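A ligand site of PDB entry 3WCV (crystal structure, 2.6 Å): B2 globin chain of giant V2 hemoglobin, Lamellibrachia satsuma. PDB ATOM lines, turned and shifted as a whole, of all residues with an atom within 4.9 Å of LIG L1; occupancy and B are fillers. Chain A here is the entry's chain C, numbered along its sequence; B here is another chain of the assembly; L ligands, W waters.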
ATOM      1  N   LEU A  40       6.956   8.405  25.140  1.00  0.00           N
ATOM      2  CA  LEU A  40       8.336   8.808  24.895  1.00  0.00           C
ATOM      3  C   LEU A  40       8.449  10.344  25.050  1.00  0.00           C
ATOM      4  O   LEU A  40       9.322  10.855  25.753  1.00  0.00           O
ATOM      5  CB  LEU A  40       8.910   8.387  23.488  1.00  0.00           C
ATOM      6  CG  LEU A  40      10.259   8.911  23.180  1.00  0.00           C
ATOM      7  CD1 LEU A  40      11.050   8.689  24.484  1.00  0.00           C
ATOM      8  CD2 LEU A  40      10.860   7.989  22.123  1.00  0.00           C
ATOM      9  N   LEU A  50      11.913  16.019  16.502  1.00  0.00           N
ATOM     10  CA  LEU A  50      12.400  15.115  15.467  1.00  0.00           C
ATOM     11  C   LEU A  50      11.294  14.652  14.541  1.00  0.00           C
ATOM     12  O   LEU A  50      11.568  14.104  13.470  1.00  0.00           O
ATOM     13  CB  LEU A  50      13.060  13.914  16.121  1.00  0.00           C
ATOM     14  CG  LEU A  50      14.154  14.265  17.130  1.00  0.00           C
ATOM     15  CD1 LEU A  50      14.496  13.061  17.979  1.00  0.00           C
ATOM     16  CD2 LEU A  50      15.372  14.773  16.388  1.00  0.00           C
ATOM     17  N   PHE A  51      10.044  14.880  14.936  1.00  0.00           N
ATOM     18  CA  PHE A  51       8.896  14.428  14.141  1.00  0.00           C
ATOM     19  C   PHE A  51       8.033  15.546  13.571  1.00  0.00           C
ATOM     20  O   PHE A  51       6.831  15.359  13.329  1.00  0.00           O
ATOM     21  CB  PHE A  51       8.044  13.493  15.003  1.00  0.00           C
ATOM     22  CG  PHE A  51       8.819  12.346  15.596  1.00  0.00           C
ATOM     23  CD1 PHE A  51       8.966  11.150  14.894  1.00  0.00           C
ATOM     24  CD2 PHE A  51       9.478  12.500  16.820  1.00  0.00           C
ATOM     25  CE1 PHE A  51       9.764  10.120  15.397  1.00  0.00           C
ATOM     26  CE2 PHE A  51      10.274  11.472  17.337  1.00  0.00           C
ATOM     27  CZ  PHE A  51      10.422  10.282  16.626  1.00  0.00           C
ATOM     28  N   ARG A  53       8.008  16.746  10.597  1.00  0.00           N
ATOM     29  CA  ARG A  53       7.520  16.432   9.260  1.00  0.00           C
ATOM     30  C   ARG A  53       6.231  15.611   9.331  1.00  0.00           C
ATOM     31  O   ARG A  53       5.380  15.698   8.447  1.00  0.00           O
ATOM     32  CB  ARG A  53       8.576  15.658   8.465  1.00  0.00           C
ATOM     33  CG  ARG A  53       8.225  15.518   6.991  1.00  0.00           C
ATOM     34  CD  ARG A  53       9.122  14.510   6.314  1.00  0.00           C
ATOM     35  NE  ARG A  53       8.662  13.146   6.543  1.00  0.00           N
ATOM     36  CZ  ARG A  53       7.644  12.574   5.891  1.00  0.00           C
ATOM     37  NH1 ARG A  53       7.298  11.322   6.155  1.00  0.00           N
ATOM     38  NH2 ARG A  53       6.984  13.249   4.964  1.00  0.00           N
ATOM     39  N   VAL A  54       6.099  14.815  10.387  1.00  0.00           N
ATOM     40  CA  VAL A  54       4.928  13.965  10.585  1.00  0.00           C
ATOM     41  C   VAL A  54       3.978  14.537  11.636  1.00  0.00           C
ATOM     42  O   VAL A  54       3.083  13.831  12.128  1.00  0.00           O
ATOM     43  CB  VAL A  54       5.366  12.534  11.011  1.00  0.00           C
ATOM     44  CG1 VAL A  54       6.133  11.865   9.860  1.00  0.00           C
ATOM     45  CG2 VAL A  54       6.238  12.589  12.254  1.00  0.00           C
ATOM     46  N   HIS A  67       2.352   7.829  10.286  1.00  0.00           N
ATOM     47  CA  HIS A  67       3.721   7.580  10.685  1.00  0.00           C
ATOM     48  C   HIS A  67       3.763   6.471  11.723  1.00  0.00           C
ATOM     49  O   HIS A  67       4.621   5.579  11.689  1.00  0.00           O
ATOM     50  CB  HIS A  67       4.338   8.841  11.290  1.00  0.00           C
ATOM     51  CG  HIS A  67       5.636   8.600  11.992  1.00  0.00           C
ATOM     52  ND1 HIS A  67       6.778   8.208  11.325  1.00  0.00           N
ATOM     53  CD2 HIS A  67       5.959   8.664  13.303  1.00  0.00           C
ATOM     54  CE1 HIS A  67       7.758   8.048  12.202  1.00  0.00           C
ATOM     55  NE2 HIS A  67       7.289   8.326  13.409  1.00  0.00           N
ATOM     56  N   ARG A  70       3.410   3.302  10.205  1.00  0.00           N
ATOM     57  CA  ARG A  70       4.670   2.902   9.558  1.00  0.00           C
ATOM     58  C   ARG A  70       5.638   2.361  10.588  1.00  0.00           C
ATOM     59  O   ARG A  70       6.357   1.396  10.323  1.00  0.00           O
ATOM     60  CB  ARG A  70       5.317   4.088   8.812  1.00  0.00           C
ATOM     61  CG  ARG A  70       4.705   4.384   7.437  1.00  0.00           C
ATOM     62  CD  ARG A  70       5.582   5.316   6.603  1.00  0.00           C
ATOM     63  NE  ARG A  70       5.753   6.642   7.227  1.00  0.00           N
ATOM     64  CZ  ARG A  70       4.890   7.651   7.094  1.00  0.00           C
ATOM     65  NH1 ARG A  70       3.791   7.495   6.376  1.00  0.00           N
ATOM     66  NH2 ARG A  70       5.104   8.816   7.697  1.00  0.00           N
ATOM     67  N   VAL A  71       5.688   2.976  11.758  1.00  0.00           N
ATOM     68  CA  VAL A  71       6.587   2.480  12.790  1.00  0.00           C
ATOM     69  C   VAL A  71       6.137   1.063  13.180  1.00  0.00           C
ATOM     70  O   VAL A  71       6.948   0.128  13.229  1.00  0.00           O
ATOM     71  CB  VAL A  71       6.583   3.387  14.037  1.00  0.00           C
ATOM     72  CG1 VAL A  71       7.534   2.809  15.089  1.00  0.00           C
ATOM     73  CG2 VAL A  71       6.990   4.796  13.658  1.00  0.00           C
ATOM     74  N   GLY A  74       7.004  -1.439  10.853  1.00  0.00           N
ATOM     75  CA  GLY A  74       8.409  -1.764  10.886  1.00  0.00           C
ATOM     76  C   GLY A  74       8.714  -2.766  11.976  1.00  0.00           C
ATOM     77  O   GLY A  74       9.499  -3.690  11.762  1.00  0.00           O
ATOM     78  N   LEU A  75       8.096  -2.570  13.135  1.00  0.00           N
ATOM     79  CA  LEU A  75       8.279  -3.454  14.274  1.00  0.00           C
ATOM     80  C   LEU A  75       7.668  -4.811  13.957  1.00  0.00           C
ATOM     81  O   LEU A  75       8.241  -5.865  14.278  1.00  0.00           O
ATOM     82  CB  LEU A  75       7.626  -2.844  15.508  1.00  0.00           C
ATOM     83  CG  LEU A  75       7.999  -3.603  16.778  1.00  0.00           C
ATOM     84  CD1 LEU A  75       9.522  -3.784  16.832  1.00  0.00           C
ATOM     85  CD2 LEU A  75       7.453  -2.862  18.034  1.00  0.00           C
ATOM     86  N   LEU A  95      16.468  -0.415   7.960  1.00  0.00           N
ATOM     87  CA  LEU A  95      15.835   0.458   8.943  1.00  0.00           C
ATOM     88  C   LEU A  95      16.886   1.372   9.542  1.00  0.00           C
ATOM     89  O   LEU A  95      16.638   2.550   9.814  1.00  0.00           O
ATOM     90  CB  LEU A  95      15.152  -0.360  10.060  1.00  0.00           C
ATOM     91  CG  LEU A  95      13.839  -1.074   9.713  1.00  0.00           C
ATOM     92  CD1 LEU A  95      13.376  -1.864  10.930  1.00  0.00           C
ATOM     93  CD2 LEU A  95      12.782  -0.056   9.291  1.00  0.00           C
ATOM     94  N   GLN A  98      17.546   4.191   7.583  1.00  0.00           N
ATOM     95  CA  GLN A  98      16.380   5.078   7.572  1.00  0.00           C
ATOM     96  C   GLN A  98      16.376   5.976   8.814  1.00  0.00           C
ATOM     97  O   GLN A  98      15.692   7.000   8.836  1.00  0.00           O
ATOM     98  CB  GLN A  98      15.076   4.268   7.491  1.00  0.00           C
ATOM     99  CG  GLN A  98      14.789   3.661   6.107  1.00  0.00           C
ATOM    100  CD  GLN A  98      13.440   2.969   6.043  1.00  0.00           C
ATOM    101  OE1 GLN A  98      13.104   2.171   6.921  1.00  0.00           O
ATOM    102  NE2 GLN A  98      12.668   3.238   5.003  1.00  0.00           N
ATOM    103  N   HIS A  99      17.144   5.600   9.834  1.00  0.00           N
ATOM    104  CA  HIS A  99      17.234   6.377  11.068  1.00  0.00           C
ATOM    105  C   HIS A  99      18.584   7.043  11.175  1.00  0.00           C
ATOM    106  O   HIS A  99      18.791   7.980  11.970  1.00  0.00           O
ATOM    107  CB  HIS A  99      17.008   5.472  12.274  1.00  0.00           C
ATOM    108  CG  HIS A  99      15.590   5.015  12.416  1.00  0.00           C
ATOM    109  ND1 HIS A  99      15.005   4.128  11.537  1.00  0.00           N
ATOM    110  CD2 HIS A  99      14.623   5.362  13.296  1.00  0.00           C
ATOM    111  CE1 HIS A  99      13.736   3.953  11.878  1.00  0.00           C
ATOM    112  NE2 HIS A  99      13.486   4.693  12.943  1.00  0.00           N
ATOM    113  N   ARG A 102      20.181  11.591  10.957  1.00  0.00           N
ATOM    114  CA  ARG A 102      18.991  12.314  11.319  1.00  0.00           C
ATOM    115  C   ARG A 102      19.352  12.730  12.729  1.00  0.00           C
ATOM    116  O   ARG A 102      19.231  11.951  13.665  1.00  0.00           O
ATOM    117  CB  ARG A 102      17.785  11.426  11.293  1.00  0.00           C
ATOM    118  CG  ARG A 102      16.925  11.641  10.091  1.00  0.00           C
ATOM    119  CD  ARG A 102      15.529  11.150  10.325  1.00  0.00           C
ATOM    120  NE  ARG A 102      15.248   9.943   9.560  1.00  0.00           N
ATOM    121  CZ  ARG A 102      14.445   9.878   8.506  1.00  0.00           C
ATOM    122  NH1 ARG A 102      14.266   8.727   7.883  1.00  0.00           N
ATOM    123  NH2 ARG A 102      13.811  10.973   8.079  1.00  0.00           N
ATOM    124  N   VAL A 105      18.335  11.433  16.478  1.00  0.00           N
ATOM    125  CA  VAL A 105      18.011  10.006  16.419  1.00  0.00           C
ATOM    126  C   VAL A 105      19.364   9.500  16.928  1.00  0.00           C
ATOM    127  O   VAL A 105      20.371   9.702  16.284  1.00  0.00           O
ATOM    128  CB  VAL A 105      17.759   9.518  14.998  1.00  0.00           C
ATOM    129  CG1 VAL A 105      17.400   8.068  15.013  1.00  0.00           C
ATOM    130  CG2 VAL A 105      16.750  10.371  14.277  1.00  0.00           C
ATOM    131  N   GLY A 109      17.717   7.592  22.465  1.00  0.00           N
ATOM    132  CA  GLY A 109      16.292   7.658  22.203  1.00  0.00           C
ATOM    133  C   GLY A 109      15.652   6.289  22.054  1.00  0.00           C
ATOM    134  O   GLY A 109      14.470   6.104  22.358  1.00  0.00           O
ATOM    135  N   PHE A 110      16.438   5.329  21.577  1.00  0.00           N
ATOM    136  CA  PHE A 110      15.948   3.979  21.387  1.00  0.00           C
ATOM    137  C   PHE A 110      15.786   3.299  22.726  1.00  0.00           C
ATOM    138  O   PHE A 110      14.845   2.527  22.926  1.00  0.00           O
ATOM    139  CB  PHE A 110      16.901   3.203  20.473  1.00  0.00           C
ATOM    140  CG  PHE A 110      16.557   3.328  19.011  1.00  0.00           C
ATOM    141  CD1 PHE A 110      15.810   2.338  18.381  1.00  0.00           C
ATOM    142  CD2 PHE A 110      16.952   4.450  18.278  1.00  0.00           C
ATOM    143  CE1 PHE A 110      15.455   2.446  17.039  1.00  0.00           C
ATOM    144  CE2 PHE A 110      16.599   4.577  16.924  1.00  0.00           C
ATOM    145  CZ  PHE A 110      15.859   3.576  16.313  1.00  0.00           C
ATOM    146  N   ILE A 113      12.464   4.800  24.064  1.00  0.00           N
ATOM    147  CA  ILE A 113      11.284   4.163  23.506  1.00  0.00           C
ATOM    148  C   ILE A 113      11.157   2.710  23.953  1.00  0.00           C
ATOM    149  O   ILE A 113      10.044   2.185  24.069  1.00  0.00           O
ATOM    150  CB  ILE A 113      11.286   4.255  21.964  1.00  0.00           C
ATOM    151  CG1 ILE A 113       9.851   4.198  21.466  1.00  0.00           C
ATOM    152  CG2 ILE A 113      12.111   3.117  21.359  1.00  0.00           C
ATOM    153  CD1 ILE A 113       9.703   4.536  20.013  1.00  0.00           C
ATOM    154  N   PHE A 137      13.450  -7.149  21.862  1.00  0.00           N
ATOM    155  CA  PHE A 137      13.239  -5.805  21.382  1.00  0.00           C
ATOM    156  C   PHE A 137      14.642  -5.247  21.192  1.00  0.00           C
ATOM    157  O   PHE A 137      14.959  -4.688  20.147  1.00  0.00           O
ATOM    158  CB  PHE A 137      12.491  -4.965  22.429  1.00  0.00           C
ATOM    159  CG  PHE A 137      12.059  -3.621  21.937  1.00  0.00           C
ATOM    160  CD1 PHE A 137      10.923  -3.479  21.136  1.00  0.00           C
ATOM    161  CD2 PHE A 137      12.794  -2.484  22.273  1.00  0.00           C
ATOM    162  CE1 PHE A 137      10.520  -2.212  20.674  1.00  0.00           C
ATOM    163  CE2 PHE A 137      12.401  -1.218  21.813  1.00  0.00           C
ATOM    164  CZ  PHE A 137      11.265  -1.084  21.007  1.00  0.00           C
ATOM    165  N   ILE A 140      16.460  -6.378  18.313  1.00  0.00           N
ATOM    166  CA  ILE A 140      15.953  -5.660  17.156  1.00  0.00           C
ATOM    167  C   ILE A 140      16.520  -4.255  17.036  1.00  0.00           C
ATOM    168  O   ILE A 140      16.944  -3.846  15.955  1.00  0.00           O
ATOM    169  CB  ILE A 140      14.407  -5.613  17.182  1.00  0.00           C
ATOM    170  CG1 ILE A 140      13.863  -6.967  16.713  1.00  0.00           C
ATOM    171  CG2 ILE A 140      13.863  -4.441  16.317  1.00  0.00           C
ATOM    172  CD1 ILE A 140      12.370  -7.103  16.826  1.00  0.00           C
ATOM    173  N   THR A 141      16.537  -3.511  18.149  1.00  0.00           N
ATOM    174  CA  THR A 141      17.077  -2.153  18.103  1.00  0.00           C
ATOM    175  C   THR A 141      18.583  -2.172  17.785  1.00  0.00           C
ATOM    176  O   THR A 141      19.050  -1.366  16.976  1.00  0.00           O
ATOM    177  CB  THR A 141      16.826  -1.368  19.437  1.00  0.00           C
ATOM    178  OG1 THR A 141      17.459  -2.032  20.533  1.00  0.00           O
ATOM    179  CG2 THR A 141      15.328  -1.222  19.703  1.00  0.00           C
ATOM    180  N   MET A 144      19.075  -1.888  14.437  1.00  0.00           N
ATOM    181  CA  MET A 144      18.598  -0.614  13.940  1.00  0.00           C
ATOM    182  C   MET A 144      19.525   0.567  14.237  1.00  0.00           C
ATOM    183  O   MET A 144      19.557   1.543  13.490  1.00  0.00           O
ATOM    184  CB  MET A 144      17.219  -0.301  14.531  1.00  0.00           C
ATOM    185  CG  MET A 144      16.101  -1.208  14.031  1.00  0.00           C
ATOM    186  SD  MET A 144      14.513  -0.684  14.746  1.00  0.00           S
ATOM    187  CE  MET A 144      14.019   0.555  13.550  1.00  0.00           C
ATOM    188  N   HIS B  90       2.886   8.682   0.716  1.00  0.00           N
ATOM    189  CA  HIS B  90       4.220   8.313   1.211  1.00  0.00           C
ATOM    190  C   HIS B  90       4.838   7.303   0.258  1.00  0.00           C
ATOM    191  O   HIS B  90       6.024   7.403  -0.100  1.00  0.00           O
ATOM    192  CB  HIS B  90       4.146   7.700   2.600  1.00  0.00           C
ATOM    193  CG  HIS B  90       5.478   7.510   3.244  1.00  0.00           C
ATOM    194  ND1 HIS B  90       6.162   8.550   3.844  1.00  0.00           N
ATOM    195  CD2 HIS B  90       6.263   6.423   3.383  1.00  0.00           C
ATOM    196  CE1 HIS B  90       7.308   8.098   4.331  1.00  0.00           C
ATOM    197  NE2 HIS B  90       7.395   6.806   4.060  1.00  0.00           N
ATOM    198  N   GLN B  94       8.170   7.379  -2.353  1.00  0.00           N
ATOM    199  CA  GLN B  94       9.238   6.384  -2.287  1.00  0.00           C
ATOM    200  C   GLN B  94       9.498   5.778  -3.662  1.00  0.00           C
ATOM    201  O   GLN B  94      10.535   5.150  -3.863  1.00  0.00           O
ATOM    202  CB  GLN B  94       8.868   5.277  -1.275  1.00  0.00           C
ATOM    203  CG  GLN B  94       8.739   5.768   0.176  1.00  0.00           C
ATOM    204  CD  GLN B  94       8.353   4.665   1.163  1.00  0.00           C
ATOM    205  OE1 GLN B  94       7.317   3.998   1.001  1.00  0.00           O
ATOM    206  NE2 GLN B  94       9.173   4.466   2.186  1.00  0.00           N
HETATM  207  C1  LIG L   1      10.944   6.880  10.721  1.00  0.00           C
HETATM  208  C2  LIG L   1      10.425   2.554  12.548  1.00  0.00           C
HETATM  209  C3  LIG L   1      12.354   4.028  16.731  1.00  0.00           C
HETATM  210  C4  LIG L   1      12.924   8.401  14.812  1.00  0.00           C
HETATM  211  C5  LIG L   1      10.630   5.571  10.834  1.00  0.00           C
HETATM  212  C6  LIG L   1      10.032   4.832   9.794  1.00  0.00           C
HETATM  213  C7  LIG L   1       9.888   3.584  10.308  1.00  0.00           C
HETATM  214  C8  LIG L   1      10.398   3.568  11.681  1.00  0.00           C
HETATM  215  C9  LIG L   1       9.280   2.361   9.607  1.00  0.00           C
HETATM  216  C10 LIG L   1       9.631   5.326   8.397  1.00  0.00           C
HETATM  217  C11 LIG L   1      10.667   5.076   7.329  1.00  0.00           C
HETATM  218  C12 LIG L   1      10.290   5.562   5.909  1.00  0.00           C
HETATM  219  O1  LIG L   1       9.267   5.086   5.329  1.00  0.00           O
HETATM  220  O2  LIG L   1      10.985   6.385   5.387  1.00  0.00           O
HETATM  221  C13 LIG L   1      10.901   2.540  13.879  1.00  0.00           C
HETATM  222  C14 LIG L   1      10.864   1.367  14.752  1.00  0.00           C
HETATM  223  C15 LIG L   1      11.438   1.820  16.003  1.00  0.00           C
HETATM  224  C16 LIG L   1      11.775   3.198  15.781  1.00  0.00           C
HETATM  225  C17 LIG L   1      10.339   0.025  14.415  1.00  0.00           C
HETATM  226  C18 LIG L   1      11.598   0.974  17.173  1.00  0.00           C
HETATM  227  C19 LIG L   1      12.592   0.135  17.382  1.00  0.00           C
HETATM  228  C20 LIG L   1      12.682   5.358  16.549  1.00  0.00           C
HETATM  229  C21 LIG L   1      13.311   6.173  17.621  1.00  0.00           C
HETATM  230  C22 LIG L   1      13.502   7.469  17.087  1.00  0.00           C
HETATM  231  C23 LIG L   1      12.948   7.352  15.680  1.00  0.00           C
HETATM  232  C24 LIG L   1      13.690   5.683  19.027  1.00  0.00           C
HETATM  233  C25 LIG L   1      14.054   8.556  17.701  1.00  0.00           C
HETATM  234  C26 LIG L   1      13.958   9.236  18.797  1.00  0.00           C
HETATM  235  C27 LIG L   1      12.420   8.374  13.509  1.00  0.00           C
HETATM  236  C28 LIG L   1      12.395   9.587  12.588  1.00  0.00           C
HETATM  237  C29 LIG L   1      11.813   9.114  11.443  1.00  0.00           C
HETATM  238  C30 LIG L   1      11.525   7.685  11.655  1.00  0.00           C
HETATM  239  C31 LIG L   1      12.900  10.964  12.943  1.00  0.00           C
HETATM  240  C32 LIG L   1      11.512   9.879  10.168  1.00  0.00           C
HETATM  241  C33 LIG L   1      10.051  10.290  10.201  1.00  0.00           C
HETATM  242  C34 LIG L   1       9.579  11.022   9.025  1.00  0.00           C
HETATM  243  O3  LIG L   1       9.674  12.277   8.986  1.00  0.00           O
HETATM  244  O4  LIG L   1       9.073  10.390   8.084  1.00  0.00           O
HETATM  245  N1  LIG L   1      10.870   4.817  11.995  1.00  0.00           N
HETATM  246  N2  LIG L   1      11.427   3.631  14.466  1.00  0.00           N
HETATM  247  N3  LIG L   1      12.489   6.112  15.410  1.00  0.00           N
HETATM  248  N4  LIG L   1      11.896   7.293  12.905  1.00  0.00           N
HETATM  249 FE1  LIG L   1      11.686   5.458  13.694  1.00  0.00          FE
HETATM  250  O1  LG2 L   2      10.159   6.128  14.347  1.00  0.00           O
HETATM  251  O2  LG2 L   2       9.336   7.020  14.592  1.00  0.00           O
HETATM  252  O   HOH W   1       7.076   8.011   8.810  1.00  0.00           O
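O4 of LIG L1 is in salt-bridge range of NH1 of Arg 53 (2.8 Å).
A ring nitrogen (NE2) of His 99 is bound to an iron atom (FE1) of LIG L1 (2.1 Å).
O1 of LIG L1 lies within hydrogen-bond range of NE2 of His 90 of chain B.
NE2 of Gln 94 of chain B sits at hydrogen-bond distance from O1 of LIG L1, at 3.2 Å.
A ring nitrogen (NE2) of His 67 is in hydrogen-bond range of an oxygen (O2) of LG2 L2.
O1 of LG2 L2 is bound to FE1 of LIG L1 (1.8 Å).
A ring nitrogen (NE2) of His 90 of chain B is in hydrogen-bond range of the side-chain amide nitrogen (NE2) of Gln 94 of chain B (3.5 Å).
A ring nitrogen (ND1) of His 99 is in hydrogen-bond range of the backbone carbonyl oxygen (O) of Leu 95 (2.9 Å).
NH1 of Arg 102 sits at hydrogen-bond distance from O of Gln 98.
Leu 50 touches LIG L1.
CZ of Phe 51 touches C4 of LIG L1 (3.6 Å).
CG1 of Val 54 touches C34 of LIG L1, 3.6 Å away.
His 67 touches LIG L1.
O of Arg 70 touches C9 of LIG L1 (3.2 Å).
Val 71 touches LIG L1.
Leu 75 touches LIG L1.
NE2 of Gln 98 touches C12 of LIG L1, at 3.4 Å.
Arg 102 touches LIG L1 (NH2 to C32, 3.3 Å).
Gly 109 touches LIG L1 (O to C24, 3.4 Å).
CE1 of Phe 110 touches C3 of LIG L1, 3.5 Å away.
CG2 of Ile 113 touches C24 of LIG L1, at 3.8 Å.
Thr 141 touches LIG L1 (CG2 to C19, 3.8 Å).
Met 144 touches LIG L1 (SD to C19, 3.4 Å).
Hydrophobic or aromatic side chains within 4 Å of LIG L1: Leu 50, Phe 51, Val 54, His 67, Val 71, His 99, Phe 110, Ile 113, Met 144 and His 90 of chain B.
Along chain A the residues within 4 Å of LIG L1 span positions 50 to 144.
The nearest printed residue that does not touch LIG L1 is Gly 74 (4.05 Å).
Water W1 lies within hydrogen-bond range of NH2 of Arg 70 (2.4 Å), ND1 of His 67 (2.5 Å) and O4 of LIG L1 (3.2 Å).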
